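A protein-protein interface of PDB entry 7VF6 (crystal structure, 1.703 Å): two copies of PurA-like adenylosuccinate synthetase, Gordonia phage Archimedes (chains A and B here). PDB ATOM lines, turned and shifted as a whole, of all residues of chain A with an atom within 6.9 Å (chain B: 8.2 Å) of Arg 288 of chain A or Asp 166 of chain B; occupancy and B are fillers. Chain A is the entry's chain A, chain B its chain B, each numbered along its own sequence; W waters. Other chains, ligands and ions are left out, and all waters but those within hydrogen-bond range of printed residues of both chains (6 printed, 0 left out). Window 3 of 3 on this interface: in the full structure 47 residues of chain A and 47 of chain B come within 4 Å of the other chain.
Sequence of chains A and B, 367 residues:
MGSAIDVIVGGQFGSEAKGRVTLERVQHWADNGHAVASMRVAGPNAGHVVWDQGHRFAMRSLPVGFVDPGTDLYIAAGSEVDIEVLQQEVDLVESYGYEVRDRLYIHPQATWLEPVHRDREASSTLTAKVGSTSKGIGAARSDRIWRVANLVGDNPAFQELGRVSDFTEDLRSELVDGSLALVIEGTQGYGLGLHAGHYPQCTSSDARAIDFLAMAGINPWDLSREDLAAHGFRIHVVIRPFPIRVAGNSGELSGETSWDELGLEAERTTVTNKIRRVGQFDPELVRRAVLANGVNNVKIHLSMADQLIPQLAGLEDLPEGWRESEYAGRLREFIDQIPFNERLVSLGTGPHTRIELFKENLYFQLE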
ATOM      1  N   GLY A  11     -22.947  11.182 -23.915  1.00  0.00           N
ATOM      2  CA  GLY A  11     -23.427   9.880 -24.320  1.00  0.00           C
ATOM      3  C   GLY A  11     -23.229   9.545 -25.781  1.00  0.00           C
ATOM      4  O   GLY A  11     -23.537   8.421 -26.190  1.00  0.00           O
ATOM      5  N   TYR A 190     -18.810   9.419 -25.119  1.00  0.00           N
ATOM      6  CA  TYR A 190     -18.470   8.006 -24.989  1.00  0.00           C
ATOM      7  C   TYR A 190     -17.941   7.425 -26.297  1.00  0.00           C
ATOM      8  O   TYR A 190     -16.941   6.695 -26.310  1.00  0.00           O
ATOM      9  CB  TYR A 190     -19.694   7.221 -24.527  1.00  0.00           C
ATOM     10  CG  TYR A 190     -19.455   5.736 -24.617  1.00  0.00           C
ATOM     11  CD1 TYR A 190     -18.598   5.112 -23.733  1.00  0.00           C
ATOM     12  CD2 TYR A 190     -20.038   4.976 -25.618  1.00  0.00           C
ATOM     13  CE1 TYR A 190     -18.345   3.757 -23.817  1.00  0.00           C
ATOM     14  CE2 TYR A 190     -19.790   3.631 -25.712  1.00  0.00           C
ATOM     15  CZ  TYR A 190     -18.946   3.025 -24.811  1.00  0.00           C
ATOM     16  OH  TYR A 190     -18.703   1.669 -24.903  1.00  0.00           O
ATOM     17  N   HIS A 195     -11.209   3.030 -26.658  1.00  0.00           N
ATOM     18  CA  HIS A 195     -11.601   1.623 -26.684  1.00  0.00           C
ATOM     19  C   HIS A 195     -13.088   1.410 -26.931  1.00  0.00           C
ATOM     20  O   HIS A 195     -13.566   0.278 -26.784  1.00  0.00           O
ATOM     21  CB  HIS A 195     -11.222   0.926 -25.370  1.00  0.00           C
ATOM     22  CG  HIS A 195      -9.757   0.937 -25.074  1.00  0.00           C
ATOM     23  ND1 HIS A 195      -9.127   2.013 -24.482  1.00  0.00           N
ATOM     24  CD2 HIS A 195      -8.801  -0.008 -25.258  1.00  0.00           C
ATOM     25  CE1 HIS A 195      -7.844   1.737 -24.333  1.00  0.00           C
ATOM     26  NE2 HIS A 195      -7.619   0.518 -24.794  1.00  0.00           N
ATOM     27  N   ALA A 196     -13.831   2.454 -27.309  1.00  0.00           N
ATOM     28  CA  ALA A 196     -15.281   2.339 -27.422  1.00  0.00           C
ATOM     29  C   ALA A 196     -15.737   1.745 -28.750  1.00  0.00           C
ATOM     30  O   ALA A 196     -16.933   1.477 -28.911  1.00  0.00           O
ATOM     31  CB  ALA A 196     -15.939   3.706 -27.210  1.00  0.00           C
ATOM     32  N   GLY A 197     -14.833   1.546 -29.703  1.00  0.00           N
ATOM     33  CA  GLY A 197     -15.176   0.747 -30.863  1.00  0.00           C
ATOM     34  C   GLY A 197     -14.849   1.363 -32.204  1.00  0.00           C
ATOM     35  O   GLY A 197     -14.840   0.656 -33.214  1.00  0.00           O
ATOM     36  N   PRO A 283     -29.956   4.936 -30.886  1.00  0.00           N
ATOM     37  CA  PRO A 283     -30.103   4.496 -29.493  1.00  0.00           C
ATOM     38  C   PRO A 283     -29.068   3.477 -29.069  1.00  0.00           C
ATOM     39  O   PRO A 283     -28.756   3.397 -27.873  1.00  0.00           O
ATOM     40  CB  PRO A 283     -31.527   3.912 -29.450  1.00  0.00           C
ATOM     41  CG  PRO A 283     -31.870   3.616 -30.858  1.00  0.00           C
ATOM     42  CD  PRO A 283     -31.151   4.632 -31.696  1.00  0.00           C
ATOM     43  N   GLU A 284     -28.531   2.681 -29.997  1.00  0.00           N
ATOM     44  CA  GLU A 284     -27.551   1.677 -29.594  1.00  0.00           C
ATOM     45  C   GLU A 284     -26.299   2.325 -29.007  1.00  0.00           C
ATOM     46  O   GLU A 284     -25.752   1.829 -28.014  1.00  0.00           O
ATOM     47  CB  GLU A 284     -27.195   0.781 -30.777  1.00  0.00           C
ATOM     48  CG  GLU A 284     -26.189  -0.312 -30.453  1.00  0.00           C
ATOM     49  CD  GLU A 284     -26.676  -1.253 -29.354  1.00  0.00           C
ATOM     50  OE1 GLU A 284     -25.820  -1.809 -28.629  1.00  0.00           O
ATOM     51  OE2 GLU A 284     -27.911  -1.430 -29.214  1.00  0.00           O
ATOM     52  N   LEU A 285     -25.832   3.433 -29.600  1.00  0.00           N
ATOM     53  CA  LEU A 285     -24.680   4.140 -29.033  1.00  0.00           C
ATOM     54  C   LEU A 285     -24.971   4.608 -27.612  1.00  0.00           C
ATOM     55  O   LEU A 285     -24.136   4.455 -26.710  1.00  0.00           O
ATOM     56  CB  LEU A 285     -24.287   5.333 -29.909  1.00  0.00           C
ATOM     57  CG  LEU A 285     -23.205   6.270 -29.338  1.00  0.00           C
ATOM     58  CD1 LEU A 285     -21.898   5.521 -29.112  1.00  0.00           C
ATOM     59  CD2 LEU A 285     -22.984   7.487 -30.264  1.00  0.00           C
ATOM     60  N   VAL A 286     -26.156   5.191 -27.401  1.00  0.00           N
ATOM     61  CA  VAL A 286     -26.522   5.686 -26.074  1.00  0.00           C
ATOM     62  C   VAL A 286     -26.683   4.527 -25.102  1.00  0.00           C
ATOM     63  O   VAL A 286     -26.313   4.630 -23.927  1.00  0.00           O
ATOM     64  CB  VAL A 286     -27.799   6.549 -26.143  1.00  0.00           C
ATOM     65  CG1 VAL A 286     -28.226   6.976 -24.728  1.00  0.00           C
ATOM     66  CG2 VAL A 286     -27.591   7.794 -27.057  1.00  0.00           C
ATOM     67  N   ARG A 287     -27.230   3.402 -25.569  1.00  0.00           N
ATOM     68  CA  ARG A 287     -27.318   2.223 -24.711  1.00  0.00           C
ATOM     69  C   ARG A 287     -25.936   1.790 -24.233  1.00  0.00           C
ATOM     70  O   ARG A 287     -25.727   1.552 -23.039  1.00  0.00           O
ATOM     71  CB  ARG A 287     -28.001   1.071 -25.455  1.00  0.00           C
ATOM     72  CG  ARG A 287     -28.402  -0.087 -24.546  1.00  0.00           C
ATOM     73  CD  ARG A 287     -28.942  -1.246 -25.365  1.00  0.00           C
ATOM     74  NE  ARG A 287     -27.865  -1.884 -26.111  1.00  0.00           N
ATOM     75  CZ  ARG A 287     -27.136  -2.893 -25.639  1.00  0.00           C
ATOM     76  NH1 ARG A 287     -27.386  -3.385 -24.430  1.00  0.00           N
ATOM     77  NH2 ARG A 287     -26.163  -3.414 -26.374  1.00  0.00           N
ATOM     78  N   ARG A 288     -24.978   1.678 -25.163  1.00  0.00           N
ATOM     79  CA  ARG A 288     -23.614   1.283 -24.805  1.00  0.00           C
ATOM     80  C   ARG A 288     -22.959   2.316 -23.895  1.00  0.00           C
ATOM     81  O   ARG A 288     -22.186   1.959 -22.998  1.00  0.00           O
ATOM     82  CB  ARG A 288     -22.776   1.082 -26.071  1.00  0.00           C
ATOM     83  CG  ARG A 288     -23.245  -0.078 -26.974  1.00  0.00           C
ATOM     84  CD  ARG A 288     -22.991  -1.420 -26.325  1.00  0.00           C
ATOM     85  NE  ARG A 288     -21.591  -1.588 -25.945  1.00  0.00           N
ATOM     86  CZ  ARG A 288     -20.682  -2.241 -26.664  1.00  0.00           C
ATOM     87  NH1 ARG A 288     -21.022  -2.812 -27.815  1.00  0.00           N
ATOM     88  NH2 ARG A 288     -19.432  -2.331 -26.224  1.00  0.00           N
ATOM     89  N   ALA A 289     -23.246   3.600 -24.119  1.00  0.00           N
ATOM     90  CA  ALA A 289     -22.685   4.651 -23.267  1.00  0.00           C
ATOM     91  C   ALA A 289     -23.206   4.536 -21.844  1.00  0.00           C
ATOM     92  O   ALA A 289     -22.434   4.641 -20.883  1.00  0.00           O
ATOM     93  CB  ALA A 289     -23.013   6.037 -23.828  1.00  0.00           C
ATOM     94  N   VAL A 290     -24.514   4.317 -21.687  1.00  0.00           N
ATOM     95  CA  VAL A 290     -25.077   4.223 -20.343  1.00  0.00           C
ATOM     96  C   VAL A 290     -24.529   3.000 -19.624  1.00  0.00           C
ATOM     97  O   VAL A 290     -24.155   3.073 -18.445  1.00  0.00           O
ATOM     98  CB  VAL A 290     -26.613   4.214 -20.394  1.00  0.00           C
ATOM     99  CG1 VAL A 290     -27.196   3.903 -19.002  1.00  0.00           C
ATOM    100  CG2 VAL A 290     -27.128   5.565 -20.901  1.00  0.00           C
ATOM    101  N   LEU A 291     -24.476   1.855 -20.321  1.00  0.00           N
ATOM    102  CA  LEU A 291     -23.905   0.652 -19.729  1.00  0.00           C
ATOM    103  C   LEU A 291     -22.462   0.875 -19.328  1.00  0.00           C
ATOM    104  O   LEU A 291     -22.043   0.474 -18.238  1.00  0.00           O
ATOM    105  CB  LEU A 291     -23.980  -0.516 -20.708  1.00  0.00           C
ATOM    106  CG  LEU A 291     -25.380  -1.085 -20.892  1.00  0.00           C
ATOM    107  CD1 LEU A 291     -25.349  -2.078 -22.025  1.00  0.00           C
ATOM    108  CD2 LEU A 291     -25.844  -1.736 -19.578  1.00  0.00           C
ATOM    109  N   ALA A 292     -21.681   1.510 -20.202  1.00  0.00           N
ATOM    110  CA  ALA A 292     -20.263   1.704 -19.907  1.00  0.00           C
ATOM    111  C   ALA A 292     -20.061   2.640 -18.722  1.00  0.00           C
ATOM    112  O   ALA A 292     -19.121   2.463 -17.933  1.00  0.00           O
ATOM    113  CB  ALA A 292     -19.548   2.243 -21.144  1.00  0.00           C
ATOM    114  N   ASN A 293     -20.920   3.651 -18.588  1.00  0.00           N
ATOM    115  CA  ASN A 293     -20.761   4.593 -17.481  1.00  0.00           C
ATOM    116  C   ASN A 293     -21.185   3.998 -16.151  1.00  0.00           C
ATOM    117  O   ASN A 293     -20.644   4.381 -15.110  1.00  0.00           O
ATOM    118  CB  ASN A 293     -21.545   5.866 -17.761  1.00  0.00           C
ATOM    119  CG  ASN A 293     -20.732   6.861 -18.544  1.00  0.00           C
ATOM    120  OD1 ASN A 293     -19.899   7.562 -17.977  1.00  0.00           O
ATOM    121  ND2 ASN A 293     -20.941   6.907 -19.853  1.00  0.00           N
ATOM    122  N   PRO A 339     -32.732   4.653 -24.637  1.00  0.00           N
ATOM    123  CA  PRO A 339     -32.418   3.559 -23.712  1.00  0.00           C
ATOM    124  C   PRO A 339     -32.452   4.042 -22.272  1.00  0.00           C
ATOM    125  O   PRO A 339     -32.049   5.166 -21.966  1.00  0.00           O
ATOM    126  CB  PRO A 339     -31.003   3.138 -24.130  1.00  0.00           C
ATOM    127  CG  PRO A 339     -30.859   3.608 -25.522  1.00  0.00           C
ATOM    128  CD  PRO A 339     -31.656   4.877 -25.615  1.00  0.00           C
ATOM    129  N   PHE A 340     -32.946   3.181 -21.386  1.00  0.00           N
ATOM    130  CA  PHE A 340     -32.993   3.471 -19.953  1.00  0.00           C
ATOM    131  C   PHE A 340     -33.722   4.780 -19.657  1.00  0.00           C
ATOM    132  O   PHE A 340     -33.309   5.561 -18.796  1.00  0.00           O
ATOM    133  CB  PHE A 340     -31.581   3.511 -19.362  1.00  0.00           C
ATOM    134  CG  PHE A 340     -30.767   2.287 -19.658  1.00  0.00           C
ATOM    135  CD1 PHE A 340     -30.978   1.114 -18.949  1.00  0.00           C
ATOM    136  CD2 PHE A 340     -29.784   2.311 -20.633  1.00  0.00           C
ATOM    137  CE1 PHE A 340     -30.220  -0.021 -19.213  1.00  0.00           C
ATOM    138  CE2 PHE A 340     -29.020   1.179 -20.904  1.00  0.00           C
ATOM    139  CZ  PHE A 340     -29.245   0.013 -20.189  1.00  0.00           C
ATOM    140  N   TYR B  74      -9.460 -13.588 -18.670  1.00  0.00           N
ATOM    141  CA  TYR B  74      -9.719 -12.431 -19.516  1.00  0.00           C
ATOM    142  C   TYR B  74      -8.481 -11.553 -19.655  1.00  0.00           C
ATOM    143  O   TYR B  74      -7.806 -11.247 -18.667  1.00  0.00           O
ATOM    144  CB  TYR B  74     -10.876 -11.596 -18.955  1.00  0.00           C
ATOM    145  CG  TYR B  74     -12.187 -12.342 -18.993  1.00  0.00           C
ATOM    146  CD1 TYR B  74     -13.022 -12.248 -20.102  1.00  0.00           C
ATOM    147  CD2 TYR B  74     -12.566 -13.179 -17.952  1.00  0.00           C
ATOM    148  CE1 TYR B  74     -14.222 -12.935 -20.162  1.00  0.00           C
ATOM    149  CE2 TYR B  74     -13.769 -13.869 -17.999  1.00  0.00           C
ATOM    150  CZ  TYR B  74     -14.593 -13.739 -19.111  1.00  0.00           C
ATOM    151  OH  TYR B  74     -15.793 -14.417 -19.177  1.00  0.00           O
ATOM    152  N   ALA B  77      -9.791  -5.045 -22.458  1.00  0.00           N
ATOM    153  CA  ALA B  77      -9.633  -4.045 -23.511  1.00  0.00           C
ATOM    154  C   ALA B  77      -8.481  -3.094 -23.200  1.00  0.00           C
ATOM    155  O   ALA B  77      -7.686  -2.756 -24.087  1.00  0.00           O
ATOM    156  CB  ALA B  77     -10.934  -3.257 -23.705  1.00  0.00           C
ATOM    157  N   TYR B 105     -10.013 -15.392 -23.041  1.00  0.00           N
ATOM    158  CA  TYR B 105     -10.751 -14.406 -23.821  1.00  0.00           C
ATOM    159  C   TYR B 105      -9.878 -13.174 -23.960  1.00  0.00           C
ATOM    160  O   TYR B 105      -9.475 -12.587 -22.953  1.00  0.00           O
ATOM    161  CB  TYR B 105     -12.078 -14.064 -23.141  1.00  0.00           C
ATOM    162  CG  TYR B 105     -12.951 -15.285 -23.026  1.00  0.00           C
ATOM    163  CD1 TYR B 105     -13.809 -15.633 -24.061  1.00  0.00           C
ATOM    164  CD2 TYR B 105     -12.871 -16.124 -21.923  1.00  0.00           C
ATOM    165  CE1 TYR B 105     -14.595 -16.763 -23.988  1.00  0.00           C
ATOM    166  CE2 TYR B 105     -13.662 -17.278 -21.842  1.00  0.00           C
ATOM    167  CZ  TYR B 105     -14.520 -17.579 -22.883  1.00  0.00           C
ATOM    168  OH  TYR B 105     -15.317 -18.699 -22.837  1.00  0.00           O
ATOM    169  N   ILE B 106      -9.563 -12.801 -25.195  1.00  0.00           N
ATOM    170  CA  ILE B 106      -8.625 -11.717 -25.465  1.00  0.00           C
ATOM    171  C   ILE B 106      -9.383 -10.594 -26.171  1.00  0.00           C
ATOM    172  O   ILE B 106      -9.937 -10.796 -27.262  1.00  0.00           O
ATOM    173  CB  ILE B 106      -7.439 -12.207 -26.308  1.00  0.00           C
ATOM    174  CG1 ILE B 106      -6.856 -13.486 -25.693  1.00  0.00           C
ATOM    175  CG2 ILE B 106      -6.365 -11.135 -26.399  1.00  0.00           C
ATOM    176  CD1 ILE B 106      -5.925 -14.235 -26.632  1.00  0.00           C
ATOM    177  N   HIS B 107      -9.406  -9.413 -25.559  1.00  0.00           N
ATOM    178  CA  HIS B 107     -10.263  -8.358 -26.086  1.00  0.00           C
ATOM    179  C   HIS B 107      -9.696  -7.783 -27.382  1.00  0.00           C
ATOM    180  O   HIS B 107      -8.513  -7.420 -27.435  1.00  0.00           O
ATOM    181  CB  HIS B 107     -10.460  -7.248 -25.057  1.00  0.00           C
ATOM    182  CG  HIS B 107     -11.705  -6.462 -25.296  1.00  0.00           C
ATOM    183  ND1 HIS B 107     -11.845  -5.605 -26.369  1.00  0.00           N
ATOM    184  CD2 HIS B 107     -12.891  -6.458 -24.648  1.00  0.00           C
ATOM    185  CE1 HIS B 107     -13.062  -5.092 -26.357  1.00  0.00           C
ATOM    186  NE2 HIS B 107     -13.715  -5.590 -25.321  1.00  0.00           N
ATOM    187  N   PRO B 108     -10.506  -7.661 -28.441  1.00  0.00           N
ATOM    188  CA  PRO B 108      -9.977  -7.137 -29.711  1.00  0.00           C
ATOM    189  C   PRO B 108      -9.569  -5.680 -29.653  1.00  0.00           C
ATOM    190  O   PRO B 108      -8.811  -5.244 -30.528  1.00  0.00           O
ATOM    191  CB  PRO B 108     -11.143  -7.342 -30.690  1.00  0.00           C
ATOM    192  CG  PRO B 108     -12.371  -7.368 -29.815  1.00  0.00           C
ATOM    193  CD  PRO B 108     -11.928  -8.041 -28.546  1.00  0.00           C
ATOM    194  N   GLN B 109     -10.053  -4.904 -28.678  1.00  0.00           N
ATOM    195  CA  GLN B 109      -9.684  -3.498 -28.583  1.00  0.00           C
ATOM    196  C   GLN B 109      -8.386  -3.272 -27.816  1.00  0.00           C
ATOM    197  O   GLN B 109      -7.971  -2.122 -27.653  1.00  0.00           O
ATOM    198  CB  GLN B 109     -10.808  -2.688 -27.928  1.00  0.00           C
ATOM    199  CG  GLN B 109     -11.992  -2.432 -28.841  1.00  0.00           C
ATOM    200  CD  GLN B 109     -11.668  -1.417 -29.930  1.00  0.00           C
ATOM    201  OE1 GLN B 109     -11.016  -0.392 -29.678  1.00  0.00           O
ATOM    202  NE2 GLN B 109     -12.101  -1.706 -31.148  1.00  0.00           N
ATOM    203  N   ARG B 163      -9.972 -17.019 -27.467  1.00  0.00           N
ATOM    204  CA  ARG B 163     -11.128 -16.455 -28.146  1.00  0.00           C
ATOM    205  C   ARG B 163     -10.960 -14.943 -28.183  1.00  0.00           C
ATOM    206  O   ARG B 163     -10.915 -14.303 -27.131  1.00  0.00           O
ATOM    207  CB  ARG B 163     -12.420 -16.837 -27.429  1.00  0.00           C
ATOM    208  N   VAL B 164     -10.847 -14.378 -29.382  1.00  0.00           N
ATOM    209  CA  VAL B 164     -10.754 -12.929 -29.544  1.00  0.00           C
ATOM    210  C   VAL B 164     -12.184 -12.411 -29.635  1.00  0.00           C
ATOM    211  O   VAL B 164     -12.854 -12.579 -30.653  1.00  0.00           O
ATOM    212  CB  VAL B 164      -9.935 -12.543 -30.774  1.00  0.00           C
ATOM    213  CG1 VAL B 164      -9.997 -11.027 -30.993  1.00  0.00           C
ATOM    214  CG2 VAL B 164      -8.489 -13.019 -30.615  1.00  0.00           C
ATOM    215  N   SER B 165     -12.674 -11.807 -28.559  1.00  0.00           N
ATOM    216  CA  SER B 165     -14.070 -11.407 -28.567  1.00  0.00           C
ATOM    217  C   SER B 165     -14.262 -10.221 -27.645  1.00  0.00           C
ATOM    218  O   SER B 165     -13.578 -10.091 -26.624  1.00  0.00           O
ATOM    219  CB  SER B 165     -14.995 -12.560 -28.154  1.00  0.00           C
ATOM    220  OG  SER B 165     -14.967 -12.769 -26.756  1.00  0.00           O
ATOM    221  N   ASP B 166     -15.166  -9.339 -28.049  1.00  0.00           N
ATOM    222  CA  ASP B 166     -15.571  -8.195 -27.239  1.00  0.00           C
ATOM    223  C   ASP B 166     -16.514  -8.694 -26.148  1.00  0.00           C
ATOM    224  O   ASP B 166     -17.742  -8.677 -26.284  1.00  0.00           O
ATOM    225  CB  ASP B 166     -16.218  -7.137 -28.121  1.00  0.00           C
ATOM    226  CG  ASP B 166     -16.691  -5.942 -27.343  1.00  0.00           C
ATOM    227  OD1 ASP B 166     -16.402  -5.857 -26.124  1.00  0.00           O
ATOM    228  OD2 ASP B 166     -17.363  -5.086 -27.958  1.00  0.00           O
ATOM    229  N   PHE B 167     -15.923  -9.139 -25.042  1.00  0.00           N
ATOM    230  CA  PHE B 167     -16.637  -9.805 -23.964  1.00  0.00           C
ATOM    231  C   PHE B 167     -17.157  -8.855 -22.888  1.00  0.00           C
ATOM    232  O   PHE B 167     -17.825  -9.312 -21.955  1.00  0.00           O
ATOM    233  CB  PHE B 167     -15.718 -10.845 -23.312  1.00  0.00           C
ATOM    234  CG  PHE B 167     -14.430 -10.262 -22.775  1.00  0.00           C
ATOM    235  CD1 PHE B 167     -13.230 -10.461 -23.443  1.00  0.00           C
ATOM    236  CD2 PHE B 167     -14.428  -9.514 -21.610  1.00  0.00           C
ATOM    237  CE1 PHE B 167     -12.043  -9.925 -22.957  1.00  0.00           C
ATOM    238  CE2 PHE B 167     -13.245  -8.968 -21.117  1.00  0.00           C
ATOM    239  CZ  PHE B 167     -12.054  -9.175 -21.792  1.00  0.00           C
ATOM    240  N   THR B 168     -16.865  -7.556 -22.972  1.00  0.00           N
ATOM    241  CA  THR B 168     -17.018  -6.703 -21.790  1.00  0.00           C
ATOM    242  C   THR B 168     -18.463  -6.656 -21.294  1.00  0.00           C
ATOM    243  O   THR B 168     -18.712  -6.735 -20.086  1.00  0.00           O
ATOM    244  CB  THR B 168     -16.489  -5.294 -22.095  1.00  0.00           C
ATOM    245  OG1 THR B 168     -15.134  -5.397 -22.564  1.00  0.00           O
ATOM    246  CG2 THR B 168     -16.521  -4.403 -20.843  1.00  0.00           C
ATOM    247  N   GLU B 169     -19.427  -6.516 -22.202  1.00  0.00           N
ATOM    248  CA  GLU B 169     -20.822  -6.430 -21.774  1.00  0.00           C
ATOM    249  C   GLU B 169     -21.380  -7.785 -21.341  1.00  0.00           C
ATOM    250  O   GLU B 169     -22.251  -7.840 -20.466  1.00  0.00           O
ATOM    251  CB  GLU B 169     -21.685  -5.832 -22.885  1.00  0.00           C
ATOM    252  CG  GLU B 169     -21.411  -4.352 -23.172  1.00  0.00           C
ATOM    253  CD  GLU B 169     -21.282  -3.502 -21.902  1.00  0.00           C
ATOM    254  OE1 GLU B 169     -20.353  -2.663 -21.850  1.00  0.00           O
ATOM    255  OE2 GLU B 169     -22.082  -3.679 -20.955  1.00  0.00           O
ATOM    256  N   ASP B 170     -20.915  -8.884 -21.944  1.00  0.00           N
ATOM    257  CA  ASP B 170     -21.252 -10.206 -21.420  1.00  0.00           C
ATOM    258  C   ASP B 170     -20.760 -10.357 -19.989  1.00  0.00           C
ATOM    259  O   ASP B 170     -21.478 -10.864 -19.115  1.00  0.00           O
ATOM    260  CB  ASP B 170     -20.630 -11.300 -22.294  1.00  0.00           C
ATOM    261  CG  ASP B 170     -21.328 -11.464 -23.638  1.00  0.00           C
ATOM    262  OD1 ASP B 170     -22.501 -11.052 -23.779  1.00  0.00           O
ATOM    263  OD2 ASP B 170     -20.692 -12.032 -24.551  1.00  0.00           O
ATOM    264  N   LEU B 171     -19.527  -9.923 -19.735  1.00  0.00           N
ATOM    265  CA  LEU B 171     -18.966  -9.996 -18.396  1.00  0.00           C
ATOM    266  C   LEU B 171     -19.735  -9.099 -17.430  1.00  0.00           C
ATOM    267  O   LEU B 171     -20.063  -9.513 -16.307  1.00  0.00           O
ATOM    268  CB  LEU B 171     -17.485  -9.614 -18.459  1.00  0.00           C
ATOM    269  CG  LEU B 171     -16.627  -9.697 -17.208  1.00  0.00           C
ATOM    270  CD1 LEU B 171     -16.673 -11.098 -16.612  1.00  0.00           C
ATOM    271  CD2 LEU B 171     -15.177  -9.290 -17.567  1.00  0.00           C
ATOM    272  N   ARG B 172     -20.046  -7.869 -17.853  1.00  0.00           N
ATOM    273  CA  ARG B 172     -20.800  -6.969 -16.992  1.00  0.00           C
ATOM    274  C   ARG B 172     -22.158  -7.573 -16.650  1.00  0.00           C
ATOM    275  O   ARG B 172     -22.605  -7.511 -15.497  1.00  0.00           O
ATOM    276  CB  ARG B 172     -20.970  -5.601 -17.661  1.00  0.00           C
ATOM    277  CG  ARG B 172     -21.288  -4.468 -16.675  1.00  0.00           C
ATOM    278  CD  ARG B 172     -21.779  -3.189 -17.378  1.00  0.00           C
ATOM    279  NE  ARG B 172     -20.964  -2.823 -18.536  1.00  0.00           N
ATOM    280  CZ  ARG B 172     -19.826  -2.136 -18.468  1.00  0.00           C
ATOM    281  NH1 ARG B 172     -19.156  -1.848 -19.580  1.00  0.00           N
ATOM    282  NH2 ARG B 172     -19.367  -1.729 -17.291  1.00  0.00           N
HETATM  283  O   HOH W   1     -12.043  -0.181 -33.647  1.00  0.00           O
HETATM  284  O   HOH W   2      -5.108  -0.514 -24.488  1.00  0.00           O
HETATM  285  O   HOH W   3     -18.061  -2.464 -23.811  1.00  0.00           O
HETATM  286  O   HOH W   4     -21.061  -0.664 -23.495  1.00  0.00           O
HETATM  287  O   HOH W   5     -17.223   0.627 -18.178  1.00  0.00           O
HETATM  288  O   HOH W   6     -12.133   2.014 -30.207  1.00  0.00           O
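Among the printed residues, merely in contact across the chains: His 195 of chain A with Gln 109 of chain B, Leu 291 of chain A with Glu 169 of chain B, Ala 292 of chain A with Arg 172 of chain B, Arg 288 of chain A with Glu 169 of chain B and Gly 197 of chain A with Gln 109 of chain B.
OD2 of Asp 166 of chain B lies within salt-bridge range of NH2 of Arg 288 of chain A, at 3.9 Å. NE2 of His 195 of chain A lies close to O of Ala 77 of chain B (3.4 Å). NE of Arg 172 of chain B sits close to O of Leu 291 of chain A (3.5 Å).
No position is printed for both chains. Of the 8 pairs that touch across the chains among the printed residues, none has its exchanged pair printed and touching as well.
Water W5 bridges O of Ala 292 of chain A and NH2 of Arg 172 of chain B. Water W4 lies within hydrogen-bond range of NE of Arg 288 of chain A (2.7 Å) and OE1 of Glu 169 of chain B (2.7 Å). Water W6 lies within hydrogen-bond range of OE1 of Gln 109 of chain B, N of Gly 197 of chain A and N of Ala 196 of chain A. Water W2 bridges a ring nitrogen (NE2) of His 195 of chain A and the backbone carbonyl oxygen (O) of Ala 77 of chain B. Water W3 lies within hydrogen-bond range of the guanidinium group (NH2) of Arg 288 of chain A (2.8 Å) and the side-chain carboxylate (OE1) of Glu 169 of chain B (3.0 Å). Water W1 lies within hydrogen-bond range of NE2 of Gln 109 of chain B and O of Gly 197 of chain A.
Of the 17 printed residues of chain B, 5 touch a printed residue of chain A. Of the 18 printed residues of chain A, 5 touch a printed residue of chain B. Among the printed residues, 8 pairs touch across the chains. Among the printed residues, Asp or Glu carboxylates within 4 Å of a Lys or Arg side-chain nitrogen of the other chain: Arg 288 of chain A with Asp 166 of chain B.
The side-chain carboxylate of Glu 169 of chain B is in salt-bridge range of the guanidinium group of Arg 172 of chain B (2.7 Å). OD1 of Asp 166 of chain B sits at hydrogen-bond distance from NE2 of His 107 of chain B, at 2.8 Å. A ring nitrogen (ND1) of His 107 of chain B lies within hydrogen-bond range of the backbone NH (N) of Gln 109 of chain B (3.0 Å).
Printed residues of chain B within 4 Å of His 195 of chain A: Ala 77 (3.2 Å) and Gln 109 (3.3 Å). Of the printed residues of chain B, Gly 197 of chain A touches Gln 109 (3.9 Å). No residue of chain B comes within 4 Å of Ala 289 of chain A. His 107 of chain B touches none of the printed residues of chain A. Of the printed residues of chain A, Gln 109 of chain B touches His 195 and Gly 197. Printed residues of chain A within 4 Å of Glu 169 of chain B: Arg 288 (3.9 Å) and Leu 291 (3.7 Å). The nearest residue of chain A that does not touch Asp 166 of chain B is Ala 196 of chain A (6.6 Å).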
